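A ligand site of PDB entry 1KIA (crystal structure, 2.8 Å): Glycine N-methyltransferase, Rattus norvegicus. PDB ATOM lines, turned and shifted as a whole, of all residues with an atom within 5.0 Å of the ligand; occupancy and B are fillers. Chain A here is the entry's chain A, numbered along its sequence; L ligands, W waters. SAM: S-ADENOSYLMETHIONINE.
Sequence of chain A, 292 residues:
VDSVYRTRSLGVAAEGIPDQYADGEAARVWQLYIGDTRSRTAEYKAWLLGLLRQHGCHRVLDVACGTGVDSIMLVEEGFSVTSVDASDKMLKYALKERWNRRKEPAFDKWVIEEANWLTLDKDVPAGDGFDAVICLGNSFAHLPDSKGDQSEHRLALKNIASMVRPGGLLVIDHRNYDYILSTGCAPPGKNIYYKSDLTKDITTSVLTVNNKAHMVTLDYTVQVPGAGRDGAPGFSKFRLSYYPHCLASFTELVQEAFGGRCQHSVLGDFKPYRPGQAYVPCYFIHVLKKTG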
ATOM      1  N   ASP A  19     -10.748 -23.552  -3.521  1.00  0.00           N
ATOM      2  CA  ASP A  19      -9.475 -23.659  -2.815  1.00  0.00           C
ATOM      3  C   ASP A  19      -8.373 -22.904  -3.544  1.00  0.00           C
ATOM      4  O   ASP A  19      -7.496 -22.307  -2.916  1.00  0.00           O
ATOM      5  CB  ASP A  19      -9.068 -25.128  -2.665  1.00  0.00           C
ATOM      6  CG  ASP A  19      -7.819 -25.307  -1.827  1.00  0.00           C
ATOM      7  OD1 ASP A  19      -7.401 -26.464  -1.622  1.00  0.00           O
ATOM      8  OD2 ASP A  19      -7.252 -24.290  -1.378  1.00  0.00           O
ATOM      9  N   TYR A  21      -6.073 -23.980  -4.636  1.00  0.00           N
ATOM     10  CA  TYR A  21      -4.888 -24.815  -4.443  1.00  0.00           C
ATOM     11  C   TYR A  21      -5.285 -26.284  -4.549  1.00  0.00           C
ATOM     12  O   TYR A  21      -4.465 -27.181  -4.444  1.00  0.00           O
ATOM     13  CB  TYR A  21      -4.265 -24.537  -3.086  1.00  0.00           C
ATOM     14  CG  TYR A  21      -3.532 -23.224  -3.039  1.00  0.00           C
ATOM     15  CD1 TYR A  21      -4.212 -22.030  -2.754  1.00  0.00           C
ATOM     16  CD2 TYR A  21      -2.170 -23.159  -3.260  1.00  0.00           C
ATOM     17  CE1 TYR A  21      -3.540 -20.821  -2.696  1.00  0.00           C
ATOM     18  CE2 TYR A  21      -1.480 -21.941  -3.204  1.00  0.00           C
ATOM     19  CZ  TYR A  21      -2.176 -20.785  -2.929  1.00  0.00           C
ATOM     20  OH  TYR A  21      -1.500 -19.583  -2.876  1.00  0.00           O
ATOM     21  N   TRP A  30       5.678 -25.359  -4.487  1.00  0.00           N
ATOM     22  CA  TRP A  30       5.780 -24.192  -3.625  1.00  0.00           C
ATOM     23  C   TRP A  30       7.204 -24.020  -3.148  1.00  0.00           C
ATOM     24  O   TRP A  30       7.744 -22.910  -3.128  1.00  0.00           O
ATOM     25  CB  TRP A  30       4.849 -24.307  -2.423  1.00  0.00           C
ATOM     26  CG  TRP A  30       4.466 -22.961  -1.926  1.00  0.00           C
ATOM     27  CD1 TRP A  30       4.795 -22.412  -0.718  1.00  0.00           C
ATOM     28  CD2 TRP A  30       3.755 -21.959  -2.640  1.00  0.00           C
ATOM     29  NE1 TRP A  30       4.326 -21.132  -0.649  1.00  0.00           N
ATOM     30  CE2 TRP A  30       3.684 -20.829  -1.814  1.00  0.00           C
ATOM     31  CE3 TRP A  30       3.158 -21.906  -3.916  1.00  0.00           C
ATOM     32  CZ2 TRP A  30       3.049 -19.640  -2.218  1.00  0.00           C
ATOM     33  CZ3 TRP A  30       2.535 -20.741  -4.309  1.00  0.00           C
ATOM     34  CH2 TRP A  30       2.483 -19.624  -3.461  1.00  0.00           C
ATOM     35  N   ILE A  34       9.336 -20.635  -3.308  1.00  0.00           N
ATOM     36  CA  ILE A  34       9.923 -19.914  -2.175  1.00  0.00           C
ATOM     37  C   ILE A  34      11.435 -19.851  -2.325  1.00  0.00           C
ATOM     38  O   ILE A  34      12.072 -18.857  -1.988  1.00  0.00           O
ATOM     39  CB  ILE A  34       9.630 -20.607  -0.831  1.00  0.00           C
ATOM     40  CG1 ILE A  34       8.188 -20.360  -0.413  1.00  0.00           C
ATOM     41  CG2 ILE A  34      10.563 -20.086   0.245  1.00  0.00           C
ATOM     42  CD1 ILE A  34       7.758 -21.212   0.732  1.00  0.00           C
ATOM     43  N   ARG A  40      14.981 -16.952   2.863  1.00  0.00           N
ATOM     44  CA  ARG A  40      13.792 -16.124   2.886  1.00  0.00           C
ATOM     45  C   ARG A  40      13.528 -15.694   4.321  1.00  0.00           C
ATOM     46  O   ARG A  40      13.390 -14.498   4.608  1.00  0.00           O
ATOM     47  CB  ARG A  40      12.610 -16.912   2.327  1.00  0.00           C
ATOM     48  CG  ARG A  40      11.480 -17.176   3.304  1.00  0.00           C
ATOM     49  CD  ARG A  40      10.124 -17.218   2.608  1.00  0.00           C
ATOM     50  NE  ARG A  40       9.036 -16.789   3.487  1.00  0.00           N
ATOM     51  CZ  ARG A  40       7.743 -16.863   3.178  1.00  0.00           C
ATOM     52  NH1 ARG A  40       7.367 -17.356   2.012  1.00  0.00           N
ATOM     53  NH2 ARG A  40       6.833 -16.440   4.034  1.00  0.00           N
ATOM     54  N   VAL A  63      -2.677 -18.488  10.528  1.00  0.00           N
ATOM     55  CA  VAL A  63      -3.854 -18.760   9.707  1.00  0.00           C
ATOM     56  C   VAL A  63      -3.549 -18.980   8.218  1.00  0.00           C
ATOM     57  O   VAL A  63      -4.422 -19.396   7.459  1.00  0.00           O
ATOM     58  CB  VAL A  63      -4.909 -17.616   9.844  1.00  0.00           C
ATOM     59  CG1 VAL A  63      -5.608 -17.710  11.173  1.00  0.00           C
ATOM     60  CG2 VAL A  63      -4.236 -16.268   9.734  1.00  0.00           C
ATOM     61  N   ALA A  64      -2.312 -18.698   7.820  1.00  0.00           N
ATOM     62  CA  ALA A  64      -1.850 -18.861   6.434  1.00  0.00           C
ATOM     63  C   ALA A  64      -0.726 -19.906   6.381  1.00  0.00           C
ATOM     64  O   ALA A  64       0.213 -19.749   5.607  1.00  0.00           O
ATOM     65  CB  ALA A  64      -1.342 -17.552   5.891  1.00  0.00           C
ATOM     66  N   CYS A  65      -0.826 -20.934   7.222  1.00  0.00           N
ATOM     67  CA  CYS A  65       0.204 -21.970   7.315  1.00  0.00           C
ATOM     68  C   CYS A  65       0.906 -22.368   6.027  1.00  0.00           C
ATOM     69  O   CYS A  65       2.129 -22.495   6.008  1.00  0.00           O
ATOM     70  CB  CYS A  65      -0.374 -23.236   7.955  1.00  0.00           C
ATOM     71  SG  CYS A  65       0.858 -24.556   8.061  1.00  0.00           S
ATOM     72  N   GLY A  66       0.147 -22.577   4.956  1.00  0.00           N
ATOM     73  CA  GLY A  66       0.787 -22.977   3.714  1.00  0.00           C
ATOM     74  C   GLY A  66       1.567 -24.261   3.951  1.00  0.00           C
ATOM     75  O   GLY A  66       1.045 -25.206   4.541  1.00  0.00           O
ATOM     76  N   THR A  67       2.807 -24.320   3.496  1.00  0.00           N
ATOM     77  CA  THR A  67       3.620 -25.518   3.679  1.00  0.00           C
ATOM     78  C   THR A  67       4.318 -25.493   5.036  1.00  0.00           C
ATOM     79  O   THR A  67       5.076 -26.414   5.365  1.00  0.00           O
ATOM     80  CB  THR A  67       4.674 -25.652   2.566  1.00  0.00           C
ATOM     81  OG1 THR A  67       5.364 -24.420   2.389  1.00  0.00           O
ATOM     82  CG2 THR A  67       4.009 -26.044   1.266  1.00  0.00           C
ATOM     83  N   VAL A  69       6.329 -22.756   6.284  1.00  0.00           N
ATOM     84  CA  VAL A  69       7.526 -21.904   6.361  1.00  0.00           C
ATOM     85  C   VAL A  69       7.721 -21.106   7.646  1.00  0.00           C
ATOM     86  O   VAL A  69       8.720 -21.270   8.342  1.00  0.00           O
ATOM     87  CB  VAL A  69       7.578 -20.885   5.213  1.00  0.00           C
ATOM     88  CG1 VAL A  69       9.017 -20.418   5.019  1.00  0.00           C
ATOM     89  CG2 VAL A  69       7.056 -21.505   3.949  1.00  0.00           C
ATOM     90  N   ASP A  70       6.775 -20.236   7.964  1.00  0.00           N
ATOM     91  CA  ASP A  70       6.896 -19.415   9.155  1.00  0.00           C
ATOM     92  C   ASP A  70       6.469 -20.113  10.431  1.00  0.00           C
ATOM     93  O   ASP A  70       6.920 -19.742  11.524  1.00  0.00           O
ATOM     94  CB  ASP A  70       6.121 -18.111   8.957  1.00  0.00           C
ATOM     95  CG  ASP A  70       6.636 -17.305   7.764  1.00  0.00           C
ATOM     96  OD1 ASP A  70       5.873 -17.142   6.784  1.00  0.00           O
ATOM     97  OD2 ASP A  70       7.792 -16.838   7.811  1.00  0.00           O
ATOM     98  N   ASP A  85      -5.013 -23.808   7.800  1.00  0.00           N
ATOM     99  CA  ASP A  85      -4.993 -23.413   6.402  1.00  0.00           C
ATOM    100  C   ASP A  85      -6.169 -24.111   5.733  1.00  0.00           C
ATOM    101  O   ASP A  85      -6.599 -25.174   6.204  1.00  0.00           O
ATOM    102  CB  ASP A  85      -3.662 -23.852   5.778  1.00  0.00           C
ATOM    103  CG  ASP A  85      -3.473 -23.321   4.379  1.00  0.00           C
ATOM    104  OD1 ASP A  85      -2.578 -22.480   4.164  1.00  0.00           O
ATOM    105  OD2 ASP A  85      -4.233 -23.760   3.497  1.00  0.00           O
ATOM    106  N   ALA A  86      -6.703 -23.531   4.663  1.00  0.00           N
ATOM    107  CA  ALA A  86      -7.843 -24.143   3.994  1.00  0.00           C
ATOM    108  C   ALA A  86      -7.456 -25.196   2.970  1.00  0.00           C
ATOM    109  O   ALA A  86      -8.275 -26.045   2.609  1.00  0.00           O
ATOM    110  CB  ALA A  86      -8.691 -23.080   3.324  1.00  0.00           C
ATOM    111  N   SER A  87      -6.217 -25.162   2.494  1.00  0.00           N
ATOM    112  CA  SER A  87      -5.782 -26.125   1.502  1.00  0.00           C
ATOM    113  C   SER A  87      -5.059 -27.306   2.127  1.00  0.00           C
ATOM    114  O   SER A  87      -3.961 -27.159   2.682  1.00  0.00           O
ATOM    115  CB  SER A  87      -4.849 -25.475   0.481  1.00  0.00           C
ATOM    116  OG  SER A  87      -4.232 -26.468  -0.326  1.00  0.00           O
ATOM    117  N   MET A  90      -1.608 -28.014   0.601  1.00  0.00           N
ATOM    118  CA  MET A  90      -0.460 -27.282   1.093  1.00  0.00           C
ATOM    119  C   MET A  90      -0.121 -27.803   2.491  1.00  0.00           C
ATOM    120  O   MET A  90       1.012 -28.139   2.789  1.00  0.00           O
ATOM    121  CB  MET A  90      -0.785 -25.795   1.137  1.00  0.00           C
ATOM    122  CG  MET A  90      -0.972 -25.194  -0.236  1.00  0.00           C
ATOM    123  SD  MET A  90       0.308 -23.998  -0.642  1.00  0.00           S
ATOM    124  CE  MET A  90       1.652 -25.032  -0.971  1.00  0.00           C
ATOM    125  N   ALA A 115      -8.593 -25.145   8.285  1.00  0.00           N
ATOM    126  CA  ALA A 115      -9.543 -24.135   8.708  1.00  0.00           C
ATOM    127  C   ALA A 115      -9.686 -23.071   7.633  1.00  0.00           C
ATOM    128  O   ALA A 115      -8.839 -22.970   6.740  1.00  0.00           O
ATOM    129  CB  ALA A 115      -9.075 -23.513  10.018  1.00  0.00           C
ATOM    130  N   ASN A 116     -10.760 -22.294   7.697  1.00  0.00           N
ATOM    131  CA  ASN A 116     -11.019 -21.253   6.717  1.00  0.00           C
ATOM    132  C   ASN A 116     -11.367 -19.934   7.381  1.00  0.00           C
ATOM    133  O   ASN A 116     -12.318 -19.877   8.170  1.00  0.00           O
ATOM    134  CB  ASN A 116     -12.165 -21.650   5.811  1.00  0.00           C
ATOM    135  CG  ASN A 116     -12.403 -20.648   4.703  1.00  0.00           C
ATOM    136  OD1 ASN A 116     -12.596 -19.457   4.947  1.00  0.00           O
ATOM    137  ND2 ASN A 116     -12.385 -21.137   3.468  1.00  0.00           N
ATOM    138  N   TRP A 117     -10.637 -18.876   7.055  1.00  0.00           N
ATOM    139  CA  TRP A 117     -10.875 -17.568   7.646  1.00  0.00           C
ATOM    140  C   TRP A 117     -12.366 -17.263   7.737  1.00  0.00           C
ATOM    141  O   TRP A 117     -12.854 -16.771   8.747  1.00  0.00           O
ATOM    142  CB  TRP A 117     -10.169 -16.482   6.824  1.00  0.00           C
ATOM    143  CG  TRP A 117      -8.709 -16.770   6.561  1.00  0.00           C
ATOM    144  CD1 TRP A 117      -7.847 -17.444   7.378  1.00  0.00           C
ATOM    145  CD2 TRP A 117      -7.966 -16.441   5.383  1.00  0.00           C
ATOM    146  NE1 TRP A 117      -6.618 -17.548   6.779  1.00  0.00           N
ATOM    147  CE2 TRP A 117      -6.660 -16.952   5.555  1.00  0.00           C
ATOM    148  CE3 TRP A 117      -8.287 -15.768   4.187  1.00  0.00           C
ATOM    149  CZ2 TRP A 117      -5.663 -16.805   4.578  1.00  0.00           C
ATOM    150  CZ3 TRP A 117      -7.288 -15.625   3.219  1.00  0.00           C
ATOM    151  CH2 TRP A 117      -6.000 -16.137   3.428  1.00  0.00           C
ATOM    152  N   LEU A 118     -13.111 -17.592   6.685  1.00  0.00           N
ATOM    153  CA  LEU A 118     -14.532 -17.335   6.666  1.00  0.00           C
ATOM    154  C   LEU A 118     -15.289 -18.011   7.811  1.00  0.00           C
ATOM    155  O   LEU A 118     -16.312 -17.496   8.259  1.00  0.00           O
ATOM    156  CB  LEU A 118     -15.115 -17.785   5.337  1.00  0.00           C
ATOM    157  CG  LEU A 118     -15.235 -16.725   4.243  1.00  0.00           C
ATOM    158  CD1 LEU A 118     -14.570 -15.430   4.649  1.00  0.00           C
ATOM    159  CD2 LEU A 118     -14.605 -17.272   2.973  1.00  0.00           C
ATOM    160  N   LEU A 136       0.952 -14.242   6.635  1.00  0.00           N
ATOM    161  CA  LEU A 136       2.010 -13.688   5.811  1.00  0.00           C
ATOM    162  C   LEU A 136       2.072 -14.271   4.412  1.00  0.00           C
ATOM    163  O   LEU A 136       1.395 -15.246   4.124  1.00  0.00           O
ATOM    164  CB  LEU A 136       3.366 -13.907   6.479  1.00  0.00           C
ATOM    165  CG  LEU A 136       3.834 -13.173   7.753  1.00  0.00           C
ATOM    166  CD1 LEU A 136       2.691 -12.405   8.386  1.00  0.00           C
ATOM    167  CD2 LEU A 136       4.411 -14.186   8.723  1.00  0.00           C
ATOM    168  N   GLY A 137       2.905 -13.667   3.572  1.00  0.00           N
ATOM    169  CA  GLY A 137       3.085 -14.142   2.206  1.00  0.00           C
ATOM    170  C   GLY A 137       1.980 -13.820   1.222  1.00  0.00           C
ATOM    171  O   GLY A 137       1.787 -14.531   0.240  1.00  0.00           O
ATOM    172  N   ASN A 138       1.260 -12.738   1.454  1.00  0.00           N
ATOM    173  CA  ASN A 138       0.179 -12.333   0.570  1.00  0.00           C
ATOM    174  C   ASN A 138      -0.868 -13.437   0.464  1.00  0.00           C
ATOM    175  O   ASN A 138      -1.226 -13.862  -0.627  1.00  0.00           O
ATOM    176  CB  ASN A 138       0.703 -12.020  -0.834  1.00  0.00           C
ATOM    177  CG  ASN A 138      -0.350 -11.371  -1.703  1.00  0.00           C
ATOM    178  OD1 ASN A 138      -1.269 -10.718  -1.197  1.00  0.00           O
ATOM    179  ND2 ASN A 138      -0.214 -11.535  -3.013  1.00  0.00           N
ATOM    180  N   SER A 139      -1.341 -13.891   1.632  1.00  0.00           N
ATOM    181  CA  SER A 139      -2.348 -14.941   1.678  1.00  0.00           C
ATOM    182  C   SER A 139      -3.752 -14.394   1.640  1.00  0.00           C
ATOM    183  O   SER A 139      -4.584 -14.893   0.895  1.00  0.00           O
ATOM    184  CB  SER A 139      -2.168 -15.777   2.936  1.00  0.00           C
ATOM    185  OG  SER A 139      -0.925 -16.460   2.909  1.00  0.00           O
ATOM    186  N   HIS A 142      -6.081 -13.390  -1.422  1.00  0.00           N
ATOM    187  CA  HIS A 142      -6.733 -14.459  -2.175  1.00  0.00           C
ATOM    188  C   HIS A 142      -8.241 -14.373  -2.060  1.00  0.00           C
ATOM    189  O   HIS A 142      -8.968 -14.744  -2.979  1.00  0.00           O
ATOM    190  CB  HIS A 142      -6.271 -15.834  -1.689  1.00  0.00           C
ATOM    191  CG  HIS A 142      -4.990 -16.307  -2.313  1.00  0.00           C
ATOM    192  ND1 HIS A 142      -3.805 -16.373  -1.626  1.00  0.00           N
ATOM    193  CD2 HIS A 142      -4.717 -16.730  -3.574  1.00  0.00           C
ATOM    194  CE1 HIS A 142      -2.855 -16.828  -2.427  1.00  0.00           C
ATOM    195  NE2 HIS A 142      -3.383 -17.048  -3.611  1.00  0.00           N
ATOM    196  N   LEU A 143      -8.718 -13.863  -0.926  1.00  0.00           N
ATOM    197  CA  LEU A 143     -10.159 -13.762  -0.702  1.00  0.00           C
ATOM    198  C   LEU A 143     -10.820 -12.837  -1.716  1.00  0.00           C
ATOM    199  O   LEU A 143     -10.460 -11.668  -1.817  1.00  0.00           O
ATOM    200  CB  LEU A 143     -10.429 -13.277   0.711  1.00  0.00           C
ATOM    201  CG  LEU A 143     -11.625 -13.904   1.432  1.00  0.00           C
ATOM    202  CD1 LEU A 143     -11.635 -15.408   1.232  1.00  0.00           C
ATOM    203  CD2 LEU A 143     -11.538 -13.577   2.911  1.00  0.00           C
ATOM    204  N   TYR A 194       9.383 -14.874  -1.698  1.00  0.00           N
ATOM    205  CA  TYR A 194       9.644 -15.873  -2.728  1.00  0.00           C
ATOM    206  C   TYR A 194      10.848 -15.462  -3.539  1.00  0.00           C
ATOM    207  O   TYR A 194      10.742 -14.668  -4.481  1.00  0.00           O
ATOM    208  CB  TYR A 194       8.411 -16.037  -3.605  1.00  0.00           C
ATOM    209  CG  TYR A 194       7.139 -16.118  -2.801  1.00  0.00           C
ATOM    210  CD1 TYR A 194       6.370 -14.974  -2.546  1.00  0.00           C
ATOM    211  CD2 TYR A 194       6.708 -17.329  -2.241  1.00  0.00           C
ATOM    212  CE1 TYR A 194       5.219 -15.034  -1.774  1.00  0.00           C
ATOM    213  CE2 TYR A 194       5.563 -17.401  -1.464  1.00  0.00           C
ATOM    214  CZ  TYR A 194       4.824 -16.254  -1.237  1.00  0.00           C
ATOM    215  OH  TYR A 194       3.676 -16.325  -0.491  1.00  0.00           O
HETATM  216  N   SAM L   1       2.236 -18.228   3.672  1.00  0.00           N
HETATM  217  CA  SAM L   1       2.863 -19.232   2.772  1.00  0.00           C
HETATM  218  C   SAM L   1       4.267 -18.801   2.443  1.00  0.00           C
HETATM  219  O   SAM L   1       4.701 -17.737   2.896  1.00  0.00           O
HETATM  220  OXT SAM L   1       4.884 -19.601   1.684  1.00  0.00           O
HETATM  221  CB  SAM L   1       2.088 -19.320   1.476  1.00  0.00           C
HETATM  222  CG  SAM L   1       0.690 -18.857   1.602  1.00  0.00           C
HETATM  223  SD  SAM L   1      -0.284 -18.907   0.084  1.00  0.00           S
HETATM  224  CE  SAM L   1       0.372 -17.580  -0.945  1.00  0.00           C
HETATM  225  C5' SAM L   1      -1.875 -18.340   0.543  1.00  0.00           C
HETATM  226  C4' SAM L   1      -2.639 -19.296   1.414  1.00  0.00           C
HETATM  227  O4' SAM L   1      -3.926 -18.714   1.720  1.00  0.00           O
HETATM  228  C3' SAM L   1      -2.968 -20.594   0.721  1.00  0.00           C
HETATM  229  O3' SAM L   1      -2.059 -21.565   1.301  1.00  0.00           O
HETATM  230  C2' SAM L   1      -4.394 -20.922   1.115  1.00  0.00           C
HETATM  231  O2' SAM L   1      -4.750 -22.216   1.540  1.00  0.00           O
HETATM  232  C1' SAM L   1      -4.737 -19.782   2.094  1.00  0.00           C
HETATM  233  N9  SAM L   1      -6.146 -19.411   2.048  1.00  0.00           N
HETATM  234  C8  SAM L   1      -6.879 -18.822   1.050  1.00  0.00           C
HETATM  235  N7  SAM L   1      -8.132 -18.616   1.355  1.00  0.00           N
HETATM  236  C5  SAM L   1      -8.239 -19.099   2.654  1.00  0.00           C
HETATM  237  C6  SAM L   1      -9.326 -19.179   3.579  1.00  0.00           C
HETATM  238  N6  SAM L   1     -10.563 -18.738   3.289  1.00  0.00           N
HETATM  239  N1  SAM L   1      -9.097 -19.724   4.820  1.00  0.00           N
HETATM  240  C2  SAM L   1      -7.851 -20.160   5.110  1.00  0.00           C
HETATM  241  N3  SAM L   1      -6.749 -20.139   4.324  1.00  0.00           N
HETATM  242  C4  SAM L   1      -7.013 -19.590   3.092  1.00  0.00           C
HETATM  243  O   HOH W   1       3.647 -18.646   6.770  1.00  0.00           O
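The side-chain carboxylate (OD2) of Asp 85 sits at hydrogen-bond distance from an oxygen (O2') of the ligand (2.5 Å).
The side-chain amide oxygen (OD1) of Asn 116 lies within hydrogen-bond range of a nitrogen (N6) of the ligand (2.7 Å).
O of the ligand lies within salt-bridge range of NH2 of Arg 40 (2.7 Å).
The backbone NH (N) of Trp 117 is in hydrogen-bond range of a nitrogen (N1) of the ligand, 2.8 Å away.
The indole nitrogen (NE1) of Trp 30 lies within hydrogen-bond range of an oxygen (OXT) of the ligand.
O of Leu 136 lies within hydrogen-bond range of N of the ligand, at 3.1 Å.
O of Ala 64 is in hydrogen-bond range of N of the ligand, 3.2 Å away.
N of Ala 86 sits at hydrogen-bond distance from N3 of the ligand, 3.4 Å away.
The backbone NH of Ser 87 is in hydrogen-bond range of an oxygen (O2') of the ligand, at 3.4 Å.
The backbone NH of Ala 115 is in hydrogen-bond range of the backbone carbonyl oxygen of Asp 85.
The indole nitrogen (NE1) of Trp 117 lies within hydrogen-bond range of the backbone carbonyl oxygen (O) of Val 63, at 2.9 Å.
The side-chain hydroxyl (OG) of Ser 139 is in hydrogen-bond range of the backbone carbonyl oxygen (O) of Leu 136 (2.9 Å).
The side-chain hydroxyl (OH) of Tyr 21 lies close to a ring nitrogen (NE2) of His 142, at 3.2 Å.
The backbone NH (N) of Tyr 21 lies close to the side-chain carboxylate (OD2) of Asp 19, 3.5 Å away.
The backbone NH (N) of Ala 86 lies within hydrogen-bond range of the backbone carbonyl oxygen (O) of Ala 115 (3.0 Å).
The side-chain hydroxyl (OG) of Ser 87 sits at hydrogen-bond distance from the backbone NH (N) of Met 90 (3.2 Å).
O of Gly 137 lies within hydrogen-bond range of OH of Tyr 194, at 2.7 Å.
Water W1 lies within hydrogen-bond range of the side-chain carboxylate of Asp 70 and a nitrogen (N) of the ligand.
The side-chain hydroxyl of Tyr 21 sits close to a sulfur (SD) of the ligand.
The side-chain hydroxyl (OG) of Ser 139 sits close to a sulfur (SD) of the ligand, at 3.8 Å.
Ile 34 touches the ligand.
O of Val 63 touches N3 of the ligand (3.97 Å).
Gly 66 touches the ligand (CA to O3', 3.99 Å).
CG2 of Val 69 touches OXT of the ligand (3.7 Å).
Met 90 touches the ligand.
O of Ala 115 touches C2 of the ligand, at 3.4 Å.
Gly 137 touches the ligand.
CE1 of His 142 touches C5' of the ligand, 3.5 Å away.
Tyr 194 touches the ligand (OH to CE, 3.6 Å).
Within 4 Å of the ligand: Tyr 21, Trp 30, Ile 34, Arg 40, Val 63, Ala 64, Gly 66, Val 69, Asp 85, Ala 86, Ser 87, Met 90, Ala 115, Asn 116, Trp 117, Leu 136, Gly 137, Ser 139, His 142 and Tyr 194.
The nearest printed residue that does not touch the ligand is Leu 143 (4.1 Å).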
